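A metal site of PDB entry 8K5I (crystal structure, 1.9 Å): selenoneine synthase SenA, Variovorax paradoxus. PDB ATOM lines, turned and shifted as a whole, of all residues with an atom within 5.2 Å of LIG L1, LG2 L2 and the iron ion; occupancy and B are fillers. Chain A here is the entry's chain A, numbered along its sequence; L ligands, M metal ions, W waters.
NE2 of His 182 binds the iron ion (2.1 Å).
The iron ion is bound by a ring nitrogen (NE2) of His 178.
The iron ion is bound by NE2 of His 82.
Water W5 is bound to the iron ion.
N2 of LG2 L2 binds the iron ion (2.2 Å).
The iron ion is bound by S1 of LIG L1.
The iron ion has six donor atoms within binding distance.
The side-chain carboxylate (OE1) of Glu 79 lies within hydrogen-bond range of an oxygen (O5) of LIG L1 (2.7 Å).
The side-chain amide nitrogen of Asn 74 sits at hydrogen-bond distance from an oxygen (O5) of LIG L1, at 3.3 Å.
OG of Ser 123 sits close to S1 of LIG L1 (3.6 Å).
ND1 of His 182 is in hydrogen-bond range of OE2 of Glu 79.
The side-chain amide nitrogen of Asn 74 is in hydrogen-bond range of the side-chain carboxylate of Glu 79 (3.0 Å).
The side-chain hydroxyl of Tyr 404 lies within hydrogen-bond range of the side-chain hydroxyl of Tyr 377, at 3.0 Å.
OH of Tyr 404 lies within hydrogen-bond range of SD of Met 181 (3.3 Å).
The side-chain sulfur (SD) of Met 189 sits at hydrogen-bond distance from the backbone NH (N) of Asn 74, 3.5 Å away.
The side-chain amide oxygen (OD1) of Asn 74 lies within hydrogen-bond range of the guanidinium group (NH1) of Arg 131 (2.9 Å).
The side-chain sulfur (SD) of Met 181 sits at hydrogen-bond distance from the side-chain hydroxyl (OH) of Tyr 377, 3.4 Å away.
The backbone carbonyl oxygen (O) of Ser 123 sits at hydrogen-bond distance from the guanidinium group (NH2) of Arg 131, at 3.3 Å.
Water W5 bridges the side-chain hydroxyl of Tyr 374 and the side-chain hydroxyl of Ser 123.
Water W7 lies within hydrogen-bond range of O1 of LIG L1 (2.5 Å) and NH2 of Arg 131 (2.9 Å).
Water W2 lies within hydrogen-bond range of O2 of LG2 L2 and OH of Tyr 188.
Water W4 lies within hydrogen-bond range of O of Tyr 377 (2.7 Å) and N1 of LG2 L2 (2.9 Å).
Water W9 lies within hydrogen-bond range of an oxygen (O5) of LIG L1 (2.9 Å) and the side-chain sulfur (SD) of Met 189 (3.6 Å).
Water W3 lies within hydrogen-bond range of the side-chain hydroxyl of Tyr 188, the guanidinium group of Arg 412 and an oxygen (O3) of LIG L1.
Merely in contact with LIG L1: Ala 185.
Hydrophobic or aromatic side chains within 4 Å of LIG L1: His 82, His 182 and Ala 185.
Six residues have an atom within 4 Å of LIG L1: Asn 74, Glu 79, His 82, Ser 123, His 182 and Ala 185.
The nearest printed residue that does not touch LIG L1 is Tyr 188 (4.02 Å).
Within 4 Å of the iron ion: His 82, His 178 and His 182.
The nearest printed residue that does not touch the iron ion is Ser 123 (4.6 Å).
Met 181 touches LG2 L2 (SD to C5, 3.7 Å).
OH of Tyr 374 touches C8 of LG2 L2 (3.2 Å).
Tyr 377 touches LG2 L2.
Tyr 404 touches LG2 L2.
OD1 of Asn 406 touches C3 of LG2 L2, at 3.4 Å.
Phe 407 touches LG2 L2 (O to C2, 3.2 Å).
Phe 408 touches LG2 L2.
Hydrophobic or aromatic side chains that line LG2 L2: His 178, Met 181, His 182, Tyr 377, Phe 407 and Phe 408.
Nine residues have an atom within 4 Å of LG2 L2: His 178, Met 181, His 182, Tyr 374, Tyr 377, Tyr 404, Asn 406, Phe 407 and Phe 408.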
ATOM      1  N   ASN A  74      23.251  -8.219 -29.794  1.00  0.00           N
ATOM      2  CA  ASN A  74      23.664  -7.088 -30.657  1.00  0.00           C
ATOM      3  C   ASN A  74      25.097  -7.366 -31.058  1.00  0.00           C
ATOM      4  O   ASN A  74      25.871  -7.936 -30.284  1.00  0.00           O
ATOM      5  CB  ASN A  74      23.566  -5.728 -29.963  1.00  0.00           C
ATOM      6  CG  ASN A  74      22.138  -5.270 -29.752  1.00  0.00           C
ATOM      7  OD1 ASN A  74      21.395  -5.026 -30.713  1.00  0.00           O
ATOM      8  ND2 ASN A  74      21.751  -5.151 -28.496  1.00  0.00           N
ATOM      9  N   TRP A  78      28.874  -2.907 -32.256  1.00  0.00           N
ATOM     10  CA  TRP A  78      27.688  -2.022 -32.095  1.00  0.00           C
ATOM     11  C   TRP A  78      27.588  -1.677 -30.608  1.00  0.00           C
ATOM     12  O   TRP A  78      27.523  -0.527 -30.297  1.00  0.00           O
ATOM     13  CB  TRP A  78      26.408  -2.658 -32.620  1.00  0.00           C
ATOM     14  CG  TRP A  78      25.296  -1.673 -32.497  1.00  0.00           C
ATOM     15  CD1 TRP A  78      24.966  -0.734 -33.427  1.00  0.00           C
ATOM     16  CD2 TRP A  78      24.455  -1.448 -31.358  1.00  0.00           C
ATOM     17  NE1 TRP A  78      23.935   0.023 -32.960  1.00  0.00           N
ATOM     18  CE2 TRP A  78      23.583  -0.401 -31.718  1.00  0.00           C
ATOM     19  CE3 TRP A  78      24.309  -2.080 -30.115  1.00  0.00           C
ATOM     20  CZ2 TRP A  78      22.621   0.080 -30.840  1.00  0.00           C
ATOM     21  CZ3 TRP A  78      23.366  -1.579 -29.225  1.00  0.00           C
ATOM     22  CH2 TRP A  78      22.504  -0.544 -29.598  1.00  0.00           C
ATOM     23  N   GLU A  79      27.623  -2.686 -29.733  1.00  0.00           N
ATOM     24  CA  GLU A  79      27.576  -2.504 -28.259  1.00  0.00           C
ATOM     25  C   GLU A  79      28.622  -1.469 -27.839  1.00  0.00           C
ATOM     26  O   GLU A  79      28.278  -0.560 -27.047  1.00  0.00           O
ATOM     27  CB  GLU A  79      27.765  -3.838 -27.528  1.00  0.00           C
ATOM     28  CG  GLU A  79      26.551  -4.768 -27.628  1.00  0.00           C
ATOM     29  CD  GLU A  79      25.456  -4.431 -26.637  1.00  0.00           C
ATOM     30  OE1 GLU A  79      24.274  -4.464 -26.999  1.00  0.00           O
ATOM     31  OE2 GLU A  79      25.796  -4.103 -25.478  1.00  0.00           O
ATOM     32  N   HIS A  82      27.700   1.978 -28.978  1.00  0.00           N
ATOM     33  CA  HIS A  82      26.504   2.380 -28.228  1.00  0.00           C
ATOM     34  C   HIS A  82      26.932   2.900 -26.859  1.00  0.00           C
ATOM     35  O   HIS A  82      26.310   3.840 -26.356  1.00  0.00           O
ATOM     36  CB  HIS A  82      25.509   1.223 -28.098  1.00  0.00           C
ATOM     37  CG  HIS A  82      24.413   1.544 -27.140  1.00  0.00           C
ATOM     38  ND1 HIS A  82      23.382   2.430 -27.452  1.00  0.00           N
ATOM     39  CD2 HIS A  82      24.178   1.152 -25.873  1.00  0.00           C
ATOM     40  CE1 HIS A  82      22.563   2.539 -26.421  1.00  0.00           C
ATOM     41  NE2 HIS A  82      23.026   1.786 -25.442  1.00  0.00           N
ATOM     42  N   PHE A  86      26.040   6.745 -25.897  1.00  0.00           N
ATOM     43  CA  PHE A  86      25.188   6.993 -24.726  1.00  0.00           C
ATOM     44  C   PHE A  86      25.891   7.973 -23.780  1.00  0.00           C
ATOM     45  O   PHE A  86      25.268   8.939 -23.302  1.00  0.00           O
ATOM     46  CB  PHE A  86      24.798   5.677 -24.030  1.00  0.00           C
ATOM     47  CG  PHE A  86      23.762   5.878 -22.963  1.00  0.00           C
ATOM     48  CD1 PHE A  86      24.134   6.232 -21.666  1.00  0.00           C
ATOM     49  CD2 PHE A  86      22.399   5.759 -23.254  1.00  0.00           C
ATOM     50  CE1 PHE A  86      23.191   6.409 -20.665  1.00  0.00           C
ATOM     51  CE2 PHE A  86      21.447   5.921 -22.245  1.00  0.00           C
ATOM     52  CZ  PHE A  86      21.845   6.250 -20.967  1.00  0.00           C
ATOM     53  N   SER A 123      19.811   3.442 -29.497  1.00  0.00           N
ATOM     54  CA  SER A 123      18.994   2.222 -29.337  1.00  0.00           C
ATOM     55  C   SER A 123      17.495   2.558 -29.481  1.00  0.00           C
ATOM     56  O   SER A 123      16.761   1.623 -29.737  1.00  0.00           O
ATOM     57  CB  SER A 123      19.314   1.519 -28.045  1.00  0.00           C
ATOM     58  OG  SER A 123      19.113   2.378 -26.934  1.00  0.00           O
ATOM     59  N   ARG A 131      21.274  -3.239 -37.113  1.00  0.00           N
ATOM     60  CA  ARG A 131      22.566  -3.061 -36.406  1.00  0.00           C
ATOM     61  C   ARG A 131      23.633  -3.994 -37.008  1.00  0.00           C
ATOM     62  O   ARG A 131      24.827  -3.715 -36.771  1.00  0.00           O
ATOM     63  CB  ARG A 131      22.359  -3.321 -34.918  1.00  0.00           C
ATOM     64  CG  ARG A 131      21.365  -2.346 -34.301  1.00  0.00           C
ATOM     65  CD  ARG A 131      20.961  -2.718 -32.913  1.00  0.00           C
ATOM     66  NE  ARG A 131      19.926  -1.801 -32.458  1.00  0.00           N
ATOM     67  CZ  ARG A 131      19.404  -1.801 -31.221  1.00  0.00           C
ATOM     68  NH1 ARG A 131      19.828  -2.674 -30.327  1.00  0.00           N
ATOM     69  NH2 ARG A 131      18.456  -0.928 -30.907  1.00  0.00           N
ATOM     70  N   HIS A 178      24.915   2.759 -16.870  1.00  0.00           N
ATOM     71  CA  HIS A 178      24.469   2.265 -18.183  1.00  0.00           C
ATOM     72  C   HIS A 178      25.562   1.360 -18.747  1.00  0.00           C
ATOM     73  O   HIS A 178      25.284   0.268 -19.267  1.00  0.00           O
ATOM     74  CB  HIS A 178      24.158   3.431 -19.140  1.00  0.00           C
ATOM     75  CG  HIS A 178      23.889   2.973 -20.528  1.00  0.00           C
ATOM     76  ND1 HIS A 178      24.820   3.085 -21.542  1.00  0.00           N
ATOM     77  CD2 HIS A 178      22.815   2.341 -21.030  1.00  0.00           C
ATOM     78  CE1 HIS A 178      24.295   2.579 -22.641  1.00  0.00           C
ATOM     79  NE2 HIS A 178      23.053   2.119 -22.362  1.00  0.00           N
ATOM     80  N   MET A 181      25.712  -1.952 -17.075  1.00  0.00           N
ATOM     81  CA  MET A 181      24.644  -2.828 -17.580  1.00  0.00           C
ATOM     82  C   MET A 181      25.053  -3.442 -18.919  1.00  0.00           C
ATOM     83  O   MET A 181      24.836  -4.643 -19.080  1.00  0.00           O
ATOM     84  CB  MET A 181      23.311  -2.081 -17.690  1.00  0.00           C
ATOM     85  CG  MET A 181      22.703  -1.822 -16.337  1.00  0.00           C
ATOM     86  SD  MET A 181      21.071  -0.985 -16.439  1.00  0.00           S
ATOM     87  CE  MET A 181      21.508   0.581 -17.160  1.00  0.00           C
ATOM     88  N   HIS A 182      25.695  -2.705 -19.824  1.00  0.00           N
ATOM     89  CA  HIS A 182      26.134  -3.241 -21.122  1.00  0.00           C
ATOM     90  C   HIS A 182      27.282  -4.248 -20.891  1.00  0.00           C
ATOM     91  O   HIS A 182      27.393  -5.164 -21.691  1.00  0.00           O
ATOM     92  CB  HIS A 182      26.484  -2.090 -22.095  1.00  0.00           C
ATOM     93  CG  HIS A 182      25.270  -1.574 -22.784  1.00  0.00           C
ATOM     94  ND1 HIS A 182      24.766  -2.168 -23.908  1.00  0.00           N
ATOM     95  CD2 HIS A 182      24.420  -0.575 -22.453  1.00  0.00           C
ATOM     96  CE1 HIS A 182      23.636  -1.565 -24.248  1.00  0.00           C
ATOM     97  NE2 HIS A 182      23.421  -0.559 -23.389  1.00  0.00           N
ATOM     98  N   ALA A 185      25.719  -7.449 -20.141  1.00  0.00           N
ATOM     99  CA  ALA A 185      25.065  -7.936 -21.380  1.00  0.00           C
ATOM    100  C   ALA A 185      26.124  -8.617 -22.267  1.00  0.00           C
ATOM    101  O   ALA A 185      25.842  -9.715 -22.830  1.00  0.00           O
ATOM    102  CB  ALA A 185      24.369  -6.811 -22.085  1.00  0.00           C
ATOM    103  N   TYR A 188      26.576 -12.111 -20.685  1.00  0.00           N
ATOM    104  CA  TYR A 188      25.532 -13.143 -20.968  1.00  0.00           C
ATOM    105  C   TYR A 188      25.434 -13.420 -22.476  1.00  0.00           C
ATOM    106  O   TYR A 188      25.182 -14.568 -22.850  1.00  0.00           O
ATOM    107  CB  TYR A 188      24.181 -12.880 -20.325  1.00  0.00           C
ATOM    108  CG  TYR A 188      23.343 -11.704 -20.764  1.00  0.00           C
ATOM    109  CD1 TYR A 188      22.663 -11.688 -21.960  1.00  0.00           C
ATOM    110  CD2 TYR A 188      23.079 -10.685 -19.860  1.00  0.00           C
ATOM    111  CE1 TYR A 188      21.849 -10.627 -22.323  1.00  0.00           C
ATOM    112  CE2 TYR A 188      22.267  -9.621 -20.193  1.00  0.00           C
ATOM    113  CZ  TYR A 188      21.622  -9.601 -21.415  1.00  0.00           C
ATOM    114  OH  TYR A 188      20.843  -8.536 -21.756  1.00  0.00           O
ATOM    115  N   MET A 189      25.655 -12.422 -23.325  1.00  0.00           N
ATOM    116  CA  MET A 189      25.687 -12.686 -24.781  1.00  0.00           C
ATOM    117  C   MET A 189      26.893 -13.594 -25.092  1.00  0.00           C
ATOM    118  O   MET A 189      26.679 -14.603 -25.826  1.00  0.00           O
ATOM    119  CB  MET A 189      25.726 -11.382 -25.581  1.00  0.00           C
ATOM    120  CG  MET A 189      24.425 -10.582 -25.471  1.00  0.00           C
ATOM    121  SD  MET A 189      24.441  -9.217 -26.635  1.00  0.00           S
ATOM    122  CE  MET A 189      25.472  -8.027 -25.769  1.00  0.00           C
ATOM    123  N   TYR A 374      16.279   9.923 -19.594  1.00  0.00           N
ATOM    124  CA  TYR A 374      16.322   8.722 -20.489  1.00  0.00           C
ATOM    125  C   TYR A 374      14.964   8.022 -20.396  1.00  0.00           C
ATOM    126  O   TYR A 374      14.762   7.027 -19.645  1.00  0.00           O
ATOM    127  CB  TYR A 374      17.526   7.838 -20.147  1.00  0.00           C
ATOM    128  CG  TYR A 374      17.615   6.561 -20.939  1.00  0.00           C
ATOM    129  CD1 TYR A 374      17.059   6.454 -22.210  1.00  0.00           C
ATOM    130  CD2 TYR A 374      18.277   5.463 -20.422  1.00  0.00           C
ATOM    131  CE1 TYR A 374      17.130   5.271 -22.934  1.00  0.00           C
ATOM    132  CE2 TYR A 374      18.376   4.288 -21.148  1.00  0.00           C
ATOM    133  CZ  TYR A 374      17.799   4.186 -22.408  1.00  0.00           C
ATOM    134  OH  TYR A 374      17.873   3.036 -23.114  1.00  0.00           O
ATOM    135  N   TYR A 377      14.017   4.153 -20.572  1.00  0.00           N
ATOM    136  CA  TYR A 377      14.729   3.153 -19.725  1.00  0.00           C
ATOM    137  C   TYR A 377      13.705   2.154 -19.132  1.00  0.00           C
ATOM    138  O   TYR A 377      13.939   0.899 -19.179  1.00  0.00           O
ATOM    139  CB  TYR A 377      15.588   3.781 -18.621  1.00  0.00           C
ATOM    140  CG  TYR A 377      16.245   2.758 -17.730  1.00  0.00           C
ATOM    141  CD1 TYR A 377      17.228   1.904 -18.220  1.00  0.00           C
ATOM    142  CD2 TYR A 377      15.859   2.612 -16.399  1.00  0.00           C
ATOM    143  CE1 TYR A 377      17.820   0.953 -17.412  1.00  0.00           C
ATOM    144  CE2 TYR A 377      16.433   1.671 -15.567  1.00  0.00           C
ATOM    145  CZ  TYR A 377      17.405   0.814 -16.077  1.00  0.00           C
ATOM    146  OH  TYR A 377      17.940  -0.152 -15.265  1.00  0.00           O
ATOM    147  N   TYR A 404      17.409  -2.178  -6.640  1.00  0.00           N
ATOM    148  CA  TYR A 404      17.472  -2.194  -8.118  1.00  0.00           C
ATOM    149  C   TYR A 404      16.393  -3.115  -8.650  1.00  0.00           C
ATOM    150  O   TYR A 404      16.262  -4.268  -8.133  1.00  0.00           O
ATOM    151  CB  TYR A 404      18.852  -2.662  -8.584  1.00  0.00           C
ATOM    152  CG  TYR A 404      18.966  -2.617 -10.080  1.00  0.00           C
ATOM    153  CD1 TYR A 404      19.313  -1.445 -10.736  1.00  0.00           C
ATOM    154  CD2 TYR A 404      18.759  -3.756 -10.814  1.00  0.00           C
ATOM    155  CE1 TYR A 404      19.366  -1.407 -12.117  1.00  0.00           C
ATOM    156  CE2 TYR A 404      18.837  -3.746 -12.196  1.00  0.00           C
ATOM    157  CZ  TYR A 404      19.162  -2.568 -12.842  1.00  0.00           C
ATOM    158  OH  TYR A 404      19.259  -2.582 -14.174  1.00  0.00           O
ATOM    159  N   ASN A 406      15.400  -5.205 -11.862  1.00  0.00           N
ATOM    160  CA  ASN A 406      15.726  -5.680 -13.219  1.00  0.00           C
ATOM    161  C   ASN A 406      14.398  -6.103 -13.851  1.00  0.00           C
ATOM    162  O   ASN A 406      13.452  -6.394 -13.114  1.00  0.00           O
ATOM    163  CB  ASN A 406      16.819  -6.726 -13.207  1.00  0.00           C
ATOM    164  CG  ASN A 406      17.601  -6.743 -14.503  1.00  0.00           C
ATOM    165  OD1 ASN A 406      17.266  -6.024 -15.451  1.00  0.00           O
ATOM    166  ND2 ASN A 406      18.654  -7.534 -14.555  1.00  0.00           N
ATOM    167  N   PHE A 407      14.333  -6.141 -15.169  1.00  0.00           N
ATOM    168  CA  PHE A 407      13.074  -6.334 -15.917  1.00  0.00           C
ATOM    169  C   PHE A 407      13.412  -6.958 -17.283  1.00  0.00           C
ATOM    170  O   PHE A 407      14.079  -6.346 -18.132  1.00  0.00           O
ATOM    171  CB  PHE A 407      12.265  -5.025 -15.980  1.00  0.00           C
ATOM    172  CG  PHE A 407      13.052  -3.801 -16.397  1.00  0.00           C
ATOM    173  CD1 PHE A 407      13.787  -3.076 -15.471  1.00  0.00           C
ATOM    174  CD2 PHE A 407      13.005  -3.345 -17.711  1.00  0.00           C
ATOM    175  CE1 PHE A 407      14.464  -1.929 -15.867  1.00  0.00           C
ATOM    176  CE2 PHE A 407      13.677  -2.191 -18.100  1.00  0.00           C
ATOM    177  CZ  PHE A 407      14.401  -1.487 -17.179  1.00  0.00           C
ATOM    178  N   PHE A 408      12.922  -8.177 -17.471  1.00  0.00           N
ATOM    179  CA  PHE A 408      12.999  -8.969 -18.718  1.00  0.00           C
ATOM    180  C   PHE A 408      11.680  -9.700 -18.922  1.00  0.00           C
ATOM    181  O   PHE A 408      10.996  -9.990 -17.950  1.00  0.00           O
ATOM    182  CB  PHE A 408      14.172  -9.946 -18.650  1.00  0.00           C
ATOM    183  CG  PHE A 408      15.525  -9.324 -18.905  1.00  0.00           C
ATOM    184  CD1 PHE A 408      15.905  -9.005 -20.199  1.00  0.00           C
ATOM    185  CD2 PHE A 408      16.389  -9.052 -17.855  1.00  0.00           C
ATOM    186  CE1 PHE A 408      17.155  -8.435 -20.452  1.00  0.00           C
ATOM    187  CE2 PHE A 408      17.638  -8.496 -18.110  1.00  0.00           C
ATOM    188  CZ  PHE A 408      18.026  -8.206 -19.402  1.00  0.00           C
ATOM    189  N   ARG A 412      12.775 -15.312 -20.944  1.00  0.00           N
ATOM    190  CA  ARG A 412      14.216 -15.128 -21.241  1.00  0.00           C
ATOM    191  C   ARG A 412      15.042 -16.087 -20.380  1.00  0.00           C
ATOM    192  O   ARG A 412      14.828 -16.106 -19.149  1.00  0.00           O
ATOM    193  CB  ARG A 412      14.653 -13.678 -20.981  1.00  0.00           C
ATOM    194  CG  ARG A 412      14.063 -12.680 -21.969  1.00  0.00           C
ATOM    195  CD  ARG A 412      14.764 -12.668 -23.303  1.00  0.00           C
ATOM    196  NE  ARG A 412      16.144 -12.239 -23.255  1.00  0.00           N
ATOM    197  CZ  ARG A 412      16.596 -11.028 -23.533  1.00  0.00           C
ATOM    198  NH1 ARG A 412      15.755 -10.055 -23.803  1.00  0.00           N
ATOM    199  NH2 ARG A 412      17.896 -10.791 -23.534  1.00  0.00           N
HETATM  200  C1  LIG L   1      20.074  -1.874 -24.659  1.00  0.00           C
HETATM  201  S1  LIG L   1      20.787  -0.285 -25.264  1.00  0.00           S
HETATM  202  C2  LIG L   1      18.963  -2.401 -25.576  1.00  0.00           C
HETATM  203  O1  LIG L   1      17.983  -1.386 -25.924  1.00  0.00           O
HETATM  204  C3  LIG L   1      18.319  -3.634 -24.909  1.00  0.00           C
HETATM  205  O2  LIG L   1      17.208  -4.078 -25.735  1.00  0.00           O
HETATM  206  C4  LIG L   1      19.308  -4.760 -24.546  1.00  0.00           C
HETATM  207  O3  LIG L   1      18.646  -5.715 -23.594  1.00  0.00           O
HETATM  208  C5  LIG L   1      20.627  -4.170 -23.966  1.00  0.00           C
HETATM  209  O4  LIG L   1      21.037  -2.961 -24.627  1.00  0.00           O
HETATM  210  C6  LIG L   1      21.810  -5.159 -23.988  1.00  0.00           C
HETATM  211  O5  LIG L   1      22.390  -5.326 -25.291  1.00  0.00           O
HETATM  212  C1  LG2 L   2      17.882  -2.999 -17.107  1.00  0.00           C
HETATM  213  C2  LG2 L   2      16.624  -4.492 -18.565  1.00  0.00           C
HETATM  214  C3  LG2 L   2      19.021  -4.847 -18.170  1.00  0.00           C
HETATM  215  O1  LG2 L   2      17.259  -3.368 -21.768  1.00  0.00           O
HETATM  216  O2  LG2 L   2      18.774  -4.815 -21.053  1.00  0.00           O
HETATM  217  C4  LG2 L   2      20.887  -0.952 -21.398  1.00  0.00           C
HETATM  218  C5  LG2 L   2      19.594  -2.289 -19.598  1.00  0.00           C
HETATM  219  N1  LG2 L   2      18.833  -0.347 -20.991  1.00  0.00           N
HETATM  220  N2  LG2 L   2      20.597   0.125 -22.181  1.00  0.00           N
HETATM  221  C6  LG2 L   2      18.069  -3.791 -20.933  1.00  0.00           C
HETATM  222  C7  LG2 L   2      19.818  -1.243 -20.627  1.00  0.00           C
HETATM  223  C8  LG2 L   2      19.362   0.450 -21.910  1.00  0.00           C
HETATM  224  C9  LG2 L   2      18.210  -2.964 -19.639  1.00  0.00           C
HETATM  225  N3  LG2 L   2      17.956  -3.809 -18.369  1.00  0.00           N
HETATM  226 FE    FE M   1      22.007   0.932 -23.718  1.00  0.00          FE
HETATM  227  O   HOH W   1      18.877  -4.872 -28.136  1.00  0.00           O
HETATM  228  O   HOH W   2      21.015  -5.955 -20.849  1.00  0.00           O
HETATM  229  O   HOH W   3      19.529  -8.467 -23.966  1.00  0.00           O
HETATM  230  O   HOH W   4      16.021  -0.286 -20.463  1.00  0.00           O
HETATM  231  O   HOH W   5      20.510   2.578 -23.910  1.00  0.00           O
HETATM  232  O   HOH W   6      22.265  -5.796 -18.432  1.00  0.00           O
HETATM  233  O   HOH W   7      17.458  -1.902 -28.335  1.00  0.00           O
HETATM  234  O   HOH W   8      21.049  -6.960 -16.320  1.00  0.00           O
HETATM  235  O   HOH W   9      21.161  -7.840 -26.085  1.00  0.00           O
